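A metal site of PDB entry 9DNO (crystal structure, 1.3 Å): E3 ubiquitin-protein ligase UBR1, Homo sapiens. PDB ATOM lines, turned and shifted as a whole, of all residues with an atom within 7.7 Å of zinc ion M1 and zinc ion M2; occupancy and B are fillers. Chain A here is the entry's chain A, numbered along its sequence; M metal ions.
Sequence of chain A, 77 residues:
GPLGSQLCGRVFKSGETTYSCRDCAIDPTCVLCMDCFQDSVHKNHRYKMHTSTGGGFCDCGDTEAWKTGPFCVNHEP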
ATOM      1  N   GLN A   6       6.694 -15.172  -7.114  1.00  0.00           N
ATOM      2  CA  GLN A   6       5.343 -15.662  -7.313  1.00  0.00           C
ATOM      3  C   GLN A   6       5.164 -16.999  -6.611  1.00  0.00           C
ATOM      4  O   GLN A   6       6.099 -17.807  -6.546  1.00  0.00           O
ATOM      5  CB  GLN A   6       5.035 -15.874  -8.798  1.00  0.00           C
ATOM      6  CG  GLN A   6       4.875 -14.595  -9.583  1.00  0.00           C
ATOM      7  CD  GLN A   6       4.978 -14.821 -11.069  1.00  0.00           C
ATOM      8  OE1 GLN A   6       5.844 -15.555 -11.556  1.00  0.00           O
ATOM      9  NE2 GLN A   6       4.094 -14.168 -11.817  1.00  0.00           N
ATOM     10  N   LEU A   7       3.970 -17.203  -6.067  1.00  0.00           N
ATOM     11  CA  LEU A   7       3.530 -18.501  -5.586  1.00  0.00           C
ATOM     12  C   LEU A   7       2.825 -19.190  -6.747  1.00  0.00           C
ATOM     13  O   LEU A   7       1.868 -18.648  -7.308  1.00  0.00           O
ATOM     14  CB  LEU A   7       2.514 -18.318  -4.454  1.00  0.00           C
ATOM     15  CG  LEU A   7       3.012 -18.033  -3.046  1.00  0.00           C
ATOM     16  CD1 LEU A   7       1.817 -17.765  -2.142  1.00  0.00           C
ATOM     17  CD2 LEU A   7       3.809 -19.201  -2.504  1.00  0.00           C
ATOM     18  N   CYS A   8       3.274 -20.398  -7.119  1.00  0.00           N
ATOM     19  CA  CYS A   8       2.655 -21.074  -8.249  1.00  0.00           C
ATOM     20  C   CYS A   8       1.173 -21.328  -7.992  1.00  0.00           C
ATOM     21  O   CYS A   8       0.315 -20.880  -8.769  1.00  0.00           O
ATOM     22  CB  CYS A   8       3.374 -22.397  -8.534  1.00  0.00           C
ATOM     23  SG  CYS A   8       2.520 -23.340  -9.834  1.00  0.00           S
ATOM     24  N   GLY A   9       0.859 -22.035  -6.909  1.00  0.00           N
ATOM     25  CA  GLY A   9      -0.516 -22.289  -6.501  1.00  0.00           C
ATOM     26  C   GLY A   9      -1.311 -23.216  -7.396  1.00  0.00           C
ATOM     27  O   GLY A   9      -2.516 -23.379  -7.148  1.00  0.00           O
ATOM     28  N   ARG A  10      -0.698 -23.834  -8.408  1.00  0.00           N
ATOM     29  CA  ARG A  10      -1.437 -24.729  -9.300  1.00  0.00           C
ATOM     30  C   ARG A  10      -2.171 -25.804  -8.507  1.00  0.00           C
ATOM     31  O   ARG A  10      -1.561 -26.542  -7.742  1.00  0.00           O
ATOM     32  CB  ARG A  10      -0.482 -25.405 -10.289  1.00  0.00           C
ATOM     33  CG  ARG A  10      -1.075 -26.676 -10.917  1.00  0.00           C
ATOM     34  CD  ARG A  10      -1.167 -26.589 -12.408  1.00  0.00           C
ATOM     35  NE  ARG A  10      -1.906 -27.718 -12.971  1.00  0.00           N
ATOM     36  CZ  ARG A  10      -2.928 -27.607 -13.801  1.00  0.00           C
ATOM     37  NH1 ARG A  10      -3.337 -26.412 -14.232  1.00  0.00           N
ATOM     38  NH2 ARG A  10      -3.551 -28.698 -14.231  1.00  0.00           N
ATOM     39  N   VAL A  11      -3.479 -25.902  -8.707  1.00  0.00           N
ATOM     40  CA  VAL A  11      -4.273 -26.952  -8.094  1.00  0.00           C
ATOM     41  C   VAL A  11      -4.288 -28.150  -9.042  1.00  0.00           C
ATOM     42  O   VAL A  11      -4.617 -28.010 -10.224  1.00  0.00           O
ATOM     43  CB  VAL A  11      -5.702 -26.464  -7.819  1.00  0.00           C
ATOM     44  CG1 VAL A  11      -6.570 -27.602  -7.278  1.00  0.00           C
ATOM     45  CG2 VAL A  11      -5.688 -25.277  -6.861  1.00  0.00           C
ATOM     46  N   PHE A  12      -3.918 -29.321  -8.545  1.00  0.00           N
ATOM     47  CA  PHE A  12      -3.767 -30.476  -9.413  1.00  0.00           C
ATOM     48  C   PHE A  12      -5.117 -31.074  -9.772  1.00  0.00           C
ATOM     49  O   PHE A  12      -6.031 -31.128  -8.948  1.00  0.00           O
ATOM     50  CB  PHE A  12      -2.931 -31.559  -8.741  1.00  0.00           C
ATOM     51  CG  PHE A  12      -1.577 -31.089  -8.312  1.00  0.00           C
ATOM     52  CD1 PHE A  12      -0.685 -30.589  -9.242  1.00  0.00           C
ATOM     53  CD2 PHE A  12      -1.206 -31.148  -6.982  1.00  0.00           C
ATOM     54  CE1 PHE A  12       0.578 -30.130  -8.831  1.00  0.00           C
ATOM     55  CE2 PHE A  12       0.042 -30.714  -6.570  1.00  0.00           C
ATOM     56  CZ  PHE A  12       0.921 -30.200  -7.507  1.00  0.00           C
ATOM     57  N   VAL A  31       5.185 -30.605  -2.576  1.00  0.00           N
ATOM     58  CA  VAL A  31       5.285 -31.080  -3.949  1.00  0.00           C
ATOM     59  C   VAL A  31       5.378 -29.899  -4.894  1.00  0.00           C
ATOM     60  O   VAL A  31       5.175 -28.742  -4.529  1.00  0.00           O
ATOM     61  CB  VAL A  31       4.113 -32.003  -4.365  1.00  0.00           C
ATOM     62  CG1 VAL A  31       4.268 -33.390  -3.764  1.00  0.00           C
ATOM     63  CG2 VAL A  31       2.804 -31.377  -3.983  1.00  0.00           C
ATOM     64  N   LEU A  32       5.645 -30.242  -6.137  1.00  0.00           N
ATOM     65  CA  LEU A  32       5.763 -29.316  -7.260  1.00  0.00           C
ATOM     66  C   LEU A  32       4.982 -29.865  -8.455  1.00  0.00           C
ATOM     67  O   LEU A  32       4.932 -31.077  -8.676  1.00  0.00           O
ATOM     68  CB  LEU A  32       7.229 -29.182  -7.739  1.00  0.00           C
ATOM     69  CG  LEU A  32       8.169 -28.587  -6.693  1.00  0.00           C
ATOM     70  CD1 LEU A  32       9.625 -28.697  -7.166  1.00  0.00           C
ATOM     71  CD2 LEU A  32       7.824 -27.119  -6.436  1.00  0.00           C
ATOM     72  N   CYS A  33       4.327 -28.969  -9.173  1.00  0.00           N
ATOM     73  CA  CYS A  33       3.783 -29.316 -10.486  1.00  0.00           C
ATOM     74  C   CYS A  33       4.901 -29.619 -11.489  1.00  0.00           C
ATOM     75  O   CYS A  33       6.082 -29.342 -11.263  1.00  0.00           O
ATOM     76  CB  CYS A  33       2.873 -28.204 -11.013  1.00  0.00           C
ATOM     77  SG  CYS A  33       3.729 -26.692 -11.501  1.00  0.00           S
ATOM     78  N   MET A  34       4.507 -30.211 -12.613  1.00  0.00           N
ATOM     79  CA  MET A  34       5.510 -30.639 -13.574  1.00  0.00           C
ATOM     80  C   MET A  34       6.330 -29.467 -14.105  1.00  0.00           C
ATOM     81  O   MET A  34       7.547 -29.585 -14.221  1.00  0.00           O
ATOM     82  CB  MET A  34       4.882 -31.423 -14.724  1.00  0.00           C
ATOM     83  CG  MET A  34       5.927 -31.929 -15.726  1.00  0.00           C
ATOM     84  SD  MET A  34       5.114 -32.971 -16.927  1.00  0.00           S
ATOM     85  CE  MET A  34       4.435 -34.158 -15.803  1.00  0.00           C
ATOM     86  N   ASP A  35       5.688 -28.347 -14.412  1.00  0.00           N
ATOM     87  CA  ASP A  35       6.441 -27.215 -14.948  1.00  0.00           C
ATOM     88  C   ASP A  35       7.420 -26.676 -13.917  1.00  0.00           C
ATOM     89  O   ASP A  35       8.595 -26.420 -14.236  1.00  0.00           O
ATOM     90  CB  ASP A  35       5.493 -26.130 -15.437  1.00  0.00           C
ATOM     91  CG  ASP A  35       4.879 -26.430 -16.794  1.00  0.00           C
ATOM     92  OD1 ASP A  35       5.364 -27.363 -17.463  1.00  0.00           O
ATOM     93  OD2 ASP A  35       3.922 -25.738 -17.189  1.00  0.00           O
ATOM     94  N   CYS A  36       6.995 -26.545 -12.666  1.00  0.00           N
ATOM     95  CA  CYS A  36       7.918 -26.011 -11.673  1.00  0.00           C
ATOM     96  C   CYS A  36       9.062 -26.983 -11.402  1.00  0.00           C
ATOM     97  O   CYS A  36      10.218 -26.581 -11.274  1.00  0.00           O
ATOM     98  CB  CYS A  36       7.182 -25.668 -10.390  1.00  0.00           C
ATOM     99  SG  CYS A  36       6.011 -24.330 -10.597  1.00  0.00           S
ATOM    100  N   PHE A  37       8.744 -28.279 -11.327  1.00  0.00           N
ATOM    101  CA  PHE A  37       9.793 -29.272 -11.118  1.00  0.00           C
ATOM    102  C   PHE A  37      10.826 -29.221 -12.236  1.00  0.00           C
ATOM    103  O   PHE A  37      12.030 -29.110 -11.971  1.00  0.00           O
ATOM    104  CB  PHE A  37       9.160 -30.667 -11.051  1.00  0.00           C
ATOM    105  CG  PHE A  37      10.174 -31.776 -11.085  1.00  0.00           C
ATOM    106  CD1 PHE A  37      10.979 -32.035 -10.015  1.00  0.00           C
ATOM    107  CD2 PHE A  37      10.313 -32.561 -12.223  1.00  0.00           C
ATOM    108  CE1 PHE A  37      11.924 -33.069 -10.062  1.00  0.00           C
ATOM    109  CE2 PHE A  37      11.257 -33.571 -12.274  1.00  0.00           C
ATOM    110  CZ  PHE A  37      12.042 -33.829 -11.195  1.00  0.00           C
ATOM    111  N   ASP A  39      11.541 -26.893 -14.195  1.00  0.00           N
ATOM    112  CA  ASP A  39      12.184 -25.590 -14.249  1.00  0.00           C
ATOM    113  C   ASP A  39      12.912 -25.235 -12.973  1.00  0.00           C
ATOM    114  O   ASP A  39      13.192 -24.059 -12.721  1.00  0.00           O
ATOM    115  CB  ASP A  39      11.159 -24.503 -14.596  1.00  0.00           C
ATOM    116  CG  ASP A  39      10.540 -24.694 -15.968  1.00  0.00           C
ATOM    117  OD1 ASP A  39      11.094 -25.487 -16.778  1.00  0.00           O
ATOM    118  OD2 ASP A  39       9.479 -24.098 -16.241  1.00  0.00           O
ATOM    119  N   SER A  40      13.239 -26.233 -12.146  1.00  0.00           N
ATOM    120  CA  SER A  40      13.817 -26.017 -10.829  1.00  0.00           C
ATOM    121  C   SER A  40      15.081 -26.841 -10.647  1.00  0.00           C
ATOM    122  O   SER A  40      15.377 -27.752 -11.421  1.00  0.00           O
ATOM    123  CB  SER A  40      12.827 -26.388  -9.697  1.00  0.00           C
ATOM    124  OG  SER A  40      12.706 -27.786  -9.566  1.00  0.00           O
ATOM    125  N   PHE A  57      -2.026 -28.748  -4.081  1.00  0.00           N
ATOM    126  CA  PHE A  57      -1.531 -27.706  -4.955  1.00  0.00           C
ATOM    127  C   PHE A  57      -0.020 -27.683  -4.897  1.00  0.00           C
ATOM    128  O   PHE A  57       0.602 -28.209  -3.966  1.00  0.00           O
ATOM    129  CB  PHE A  57      -2.011 -26.322  -4.490  1.00  0.00           C
ATOM    130  CG  PHE A  57      -1.830 -26.079  -3.012  1.00  0.00           C
ATOM    131  CD1 PHE A  57      -2.569 -26.798  -2.062  1.00  0.00           C
ATOM    132  CD2 PHE A  57      -0.881 -25.182  -2.567  1.00  0.00           C
ATOM    133  CE1 PHE A  57      -2.392 -26.584  -0.707  1.00  0.00           C
ATOM    134  CE2 PHE A  57      -0.700 -24.952  -1.214  1.00  0.00           C
ATOM    135  CZ  PHE A  57      -1.453 -25.662  -0.277  1.00  0.00           C
ATOM    136  N   CYS A  58       0.554 -27.055  -5.917  1.00  0.00           N
ATOM    137  CA  CYS A  58       1.988 -26.872  -6.002  1.00  0.00           C
ATOM    138  C   CYS A  58       2.508 -25.934  -4.921  1.00  0.00           C
ATOM    139  O   CYS A  58       1.925 -24.868  -4.674  1.00  0.00           O
ATOM    140  CB  CYS A  58       2.318 -26.302  -7.376  1.00  0.00           C
ATOM    141  SG  CYS A  58       4.096 -26.030  -7.660  1.00  0.00           S
ATOM    142  N   ASP A  59       3.612 -26.320  -4.292  1.00  0.00           N
ATOM    143  CA  ASP A  59       4.240 -25.521  -3.235  1.00  0.00           C
ATOM    144  C   ASP A  59       5.394 -24.661  -3.758  1.00  0.00           C
ATOM    145  O   ASP A  59       6.145 -24.123  -2.944  1.00  0.00           O
ATOM    146  CB  ASP A  59       4.753 -26.414  -2.118  1.00  0.00           C
ATOM    147  CG  ASP A  59       3.636 -27.210  -1.446  1.00  0.00           C
ATOM    148  OD1 ASP A  59       2.689 -26.547  -0.948  1.00  0.00           O
ATOM    149  OD2 ASP A  59       3.707 -28.464  -1.420  1.00  0.00           O
ATOM    150  N   CYS A  60       5.551 -24.529  -5.063  1.00  0.00           N
ATOM    151  CA  CYS A  60       6.590 -23.656  -5.570  1.00  0.00           C
ATOM    152  C   CYS A  60       6.361 -22.231  -5.090  1.00  0.00           C
ATOM    153  O   CYS A  60       5.248 -21.704  -5.178  1.00  0.00           O
ATOM    154  CB  CYS A  60       6.598 -23.663  -7.089  1.00  0.00           C
ATOM    155  SG  CYS A  60       8.007 -22.742  -7.749  1.00  0.00           S
ATOM    156  N   GLY A  61       7.428 -21.611  -4.566  1.00  0.00           N
ATOM    157  CA  GLY A  61       7.376 -20.256  -4.072  1.00  0.00           C
ATOM    158  C   GLY A  61       7.014 -20.136  -2.613  1.00  0.00           C
ATOM    159  O   GLY A  61       7.009 -19.026  -2.059  1.00  0.00           O
ATOM    160  N   PRO A  70      13.557 -22.792  -3.265  1.00  0.00           N
ATOM    161  CA  PRO A  70      12.107 -22.597  -3.076  1.00  0.00           C
ATOM    162  C   PRO A  70      11.370 -22.115  -4.310  1.00  0.00           C
ATOM    163  O   PRO A  70      10.140 -22.252  -4.368  1.00  0.00           O
ATOM    164  CB  PRO A  70      12.034 -21.544  -1.962  1.00  0.00           C
ATOM    165  CG  PRO A  70      13.323 -20.824  -2.087  1.00  0.00           C
ATOM    166  CD  PRO A  70      14.331 -21.876  -2.419  1.00  0.00           C
ATOM    167  N   PHE A  71      12.057 -21.540  -5.286  1.00  0.00           N
ATOM    168  CA  PHE A  71      11.419 -21.049  -6.493  1.00  0.00           C
ATOM    169  C   PHE A  71      12.009 -21.712  -7.728  1.00  0.00           C
ATOM    170  O   PHE A  71      13.226 -21.831  -7.844  1.00  0.00           O
ATOM    171  CB  PHE A  71      11.670 -19.543  -6.672  1.00  0.00           C
ATOM    172  CG  PHE A  71      11.077 -18.694  -5.592  1.00  0.00           C
ATOM    173  CD1 PHE A  71       9.739 -18.326  -5.643  1.00  0.00           C
ATOM    174  CD2 PHE A  71      11.858 -18.228  -4.562  1.00  0.00           C
ATOM    175  CE1 PHE A  71       9.190 -17.528  -4.638  1.00  0.00           C
ATOM    176  CE2 PHE A  71      11.324 -17.424  -3.569  1.00  0.00           C
ATOM    177  CZ  PHE A  71       9.987 -17.079  -3.614  1.00  0.00           C
ATOM    178  N   CYS A  72      11.157 -22.111  -8.658  1.00  0.00           N
ATOM    179  CA  CYS A  72      11.613 -22.441  -9.997  1.00  0.00           C
ATOM    180  C   CYS A  72      12.004 -21.145 -10.710  1.00  0.00           C
ATOM    181  O   CYS A  72      11.724 -20.034 -10.247  1.00  0.00           O
ATOM    182  CB  CYS A  72      10.541 -23.224 -10.770  1.00  0.00           C
ATOM    183  SG  CYS A  72       9.218 -22.212 -11.312  1.00  0.00           S
ATOM    184  N   VAL A  73      12.656 -21.287 -11.868  1.00  0.00           N
ATOM    185  CA  VAL A  73      13.112 -20.090 -12.588  1.00  0.00           C
ATOM    186  C   VAL A  73      11.942 -19.236 -13.092  1.00  0.00           C
ATOM    187  O   VAL A  73      12.094 -18.026 -13.253  1.00  0.00           O
ATOM    188  CB  VAL A  73      14.148 -20.402 -13.682  1.00  0.00           C
ATOM    189  CG1 VAL A  73      15.415 -21.010 -13.090  1.00  0.00           C
ATOM    190  CG2 VAL A  73      13.554 -21.289 -14.727  1.00  0.00           C
ATOM    191  N   ASN A  74      10.762 -19.836 -13.325  1.00  0.00           N
ATOM    192  CA  ASN A  74       9.607 -19.029 -13.718  1.00  0.00           C
ATOM    193  C   ASN A  74       9.050 -18.179 -12.575  1.00  0.00           C
ATOM    194  O   ASN A  74       8.517 -17.086 -12.829  1.00  0.00           O
ATOM    195  CB  ASN A  74       8.504 -19.891 -14.335  1.00  0.00           C
ATOM    196  CG  ASN A  74       8.608 -19.937 -15.841  1.00  0.00           C
ATOM    197  OD1 ASN A  74       8.921 -18.918 -16.465  1.00  0.00           O
ATOM    198  ND2 ASN A  74       8.328 -21.091 -16.419  1.00  0.00           N
ATOM    199  N   HIS A  75       9.129 -18.638 -11.340  1.00  0.00           N
ATOM    200  CA  HIS A  75       8.430 -17.986 -10.247  1.00  0.00           C
ATOM    201  C   HIS A  75       9.370 -17.200  -9.349  1.00  0.00           C
ATOM    202  O   HIS A  75       8.895 -16.507  -8.445  1.00  0.00           O
ATOM    203  CB  HIS A  75       7.600 -19.030  -9.488  1.00  0.00           C
ATOM    204  CG  HIS A  75       6.485 -19.605 -10.321  1.00  0.00           C
ATOM    205  ND1 HIS A  75       6.213 -20.950 -10.418  1.00  0.00           N
ATOM    206  CD2 HIS A  75       5.591 -18.986 -11.133  1.00  0.00           C
ATOM    207  CE1 HIS A  75       5.182 -21.132 -11.232  1.00  0.00           C
ATOM    208  NE2 HIS A  75       4.776 -19.950 -11.667  1.00  0.00           N
ATOM    209  N   GLU A  76      10.679 -17.285  -9.586  1.00  0.00           N
ATOM    210  CA  GLU A  76      11.629 -16.587  -8.759  1.00  0.00           C
ATOM    211  C   GLU A  76      11.510 -15.076  -8.975  1.00  0.00           C
ATOM    212  O   GLU A  76      11.018 -14.624 -10.003  1.00  0.00           O
ATOM    213  CB  GLU A  76      13.047 -17.027  -9.121  1.00  0.00           C
ATOM    214  CG  GLU A  76      13.417 -16.751 -10.540  1.00  0.00           C
ATOM    215  CD  GLU A  76      14.884 -16.938 -10.771  1.00  0.00           C
ATOM    216  OE1 GLU A  76      15.439 -17.910 -10.204  1.00  0.00           O
ATOM    217  OE2 GLU A  76      15.483 -16.140 -11.530  1.00  0.00           O
HETATM  218 ZN    ZN M   1       3.928 -25.120  -9.811  1.00  0.00          ZN
HETATM  219 ZN    ZN M   2       7.401 -22.490  -9.928  1.00  0.00          ZN
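The backbone NH (N) of Gln 6 sits at hydrogen-bond distance from the backbone carbonyl oxygen (O) of His 75 (2.9 Å). O of Cys 60 lies within hydrogen-bond range of N of Cys 8, 3.1 Å away. The side-chain sulfur of Cys 8 sits close to the backbone NH of Arg 10 (3.6 Å). The side-chain sulfur (SG) of Cys 58 sits close to the backbone NH (N) of Cys 60 (3.3 Å). SG of Cys 72 sits close to N of Asn 74 (3.5 Å). The backbone carbonyl oxygen (O) of Arg 10 is in hydrogen-bond range of the backbone NH (N) of Cys 58. The backbone carbonyl oxygen (O) of Cys 36 sits close to the side-chain hydroxyl (OG) of Ser 40.
Of the 28 residues printed, 4 come within 4 Å of zinc ion M1. The nearest printed residue that does not touch zinc ion M1 is Cys 60 (4.1 Å).
Within 4 Å of zinc ion M2: Cys 36, Cys 60, Cys 72 and His 75. Along chain A the residues within 4 Å of zinc ion M2 span positions 36 to 75.
Zinc ion M1 is bound by SG of Cys 8 (2.3 Å). The side-chain sulfur (SG) of Cys 33 is bound to zinc ion M1 (2.3 Å). The side-chain sulfur (SG) of Cys 58 is bound to zinc ion M1 (2.3 Å). SG of Cys 36 binds zinc ion M1, at 2.4 Å. Zinc ion M1 has four donor atoms within binding distance.
Zinc ion M2 is bound by ND1 of His 75, SG of Cys 60, SG of Cys 72 and SG of Cys 36. Zinc ion M2 has four donor atoms within binding distance.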
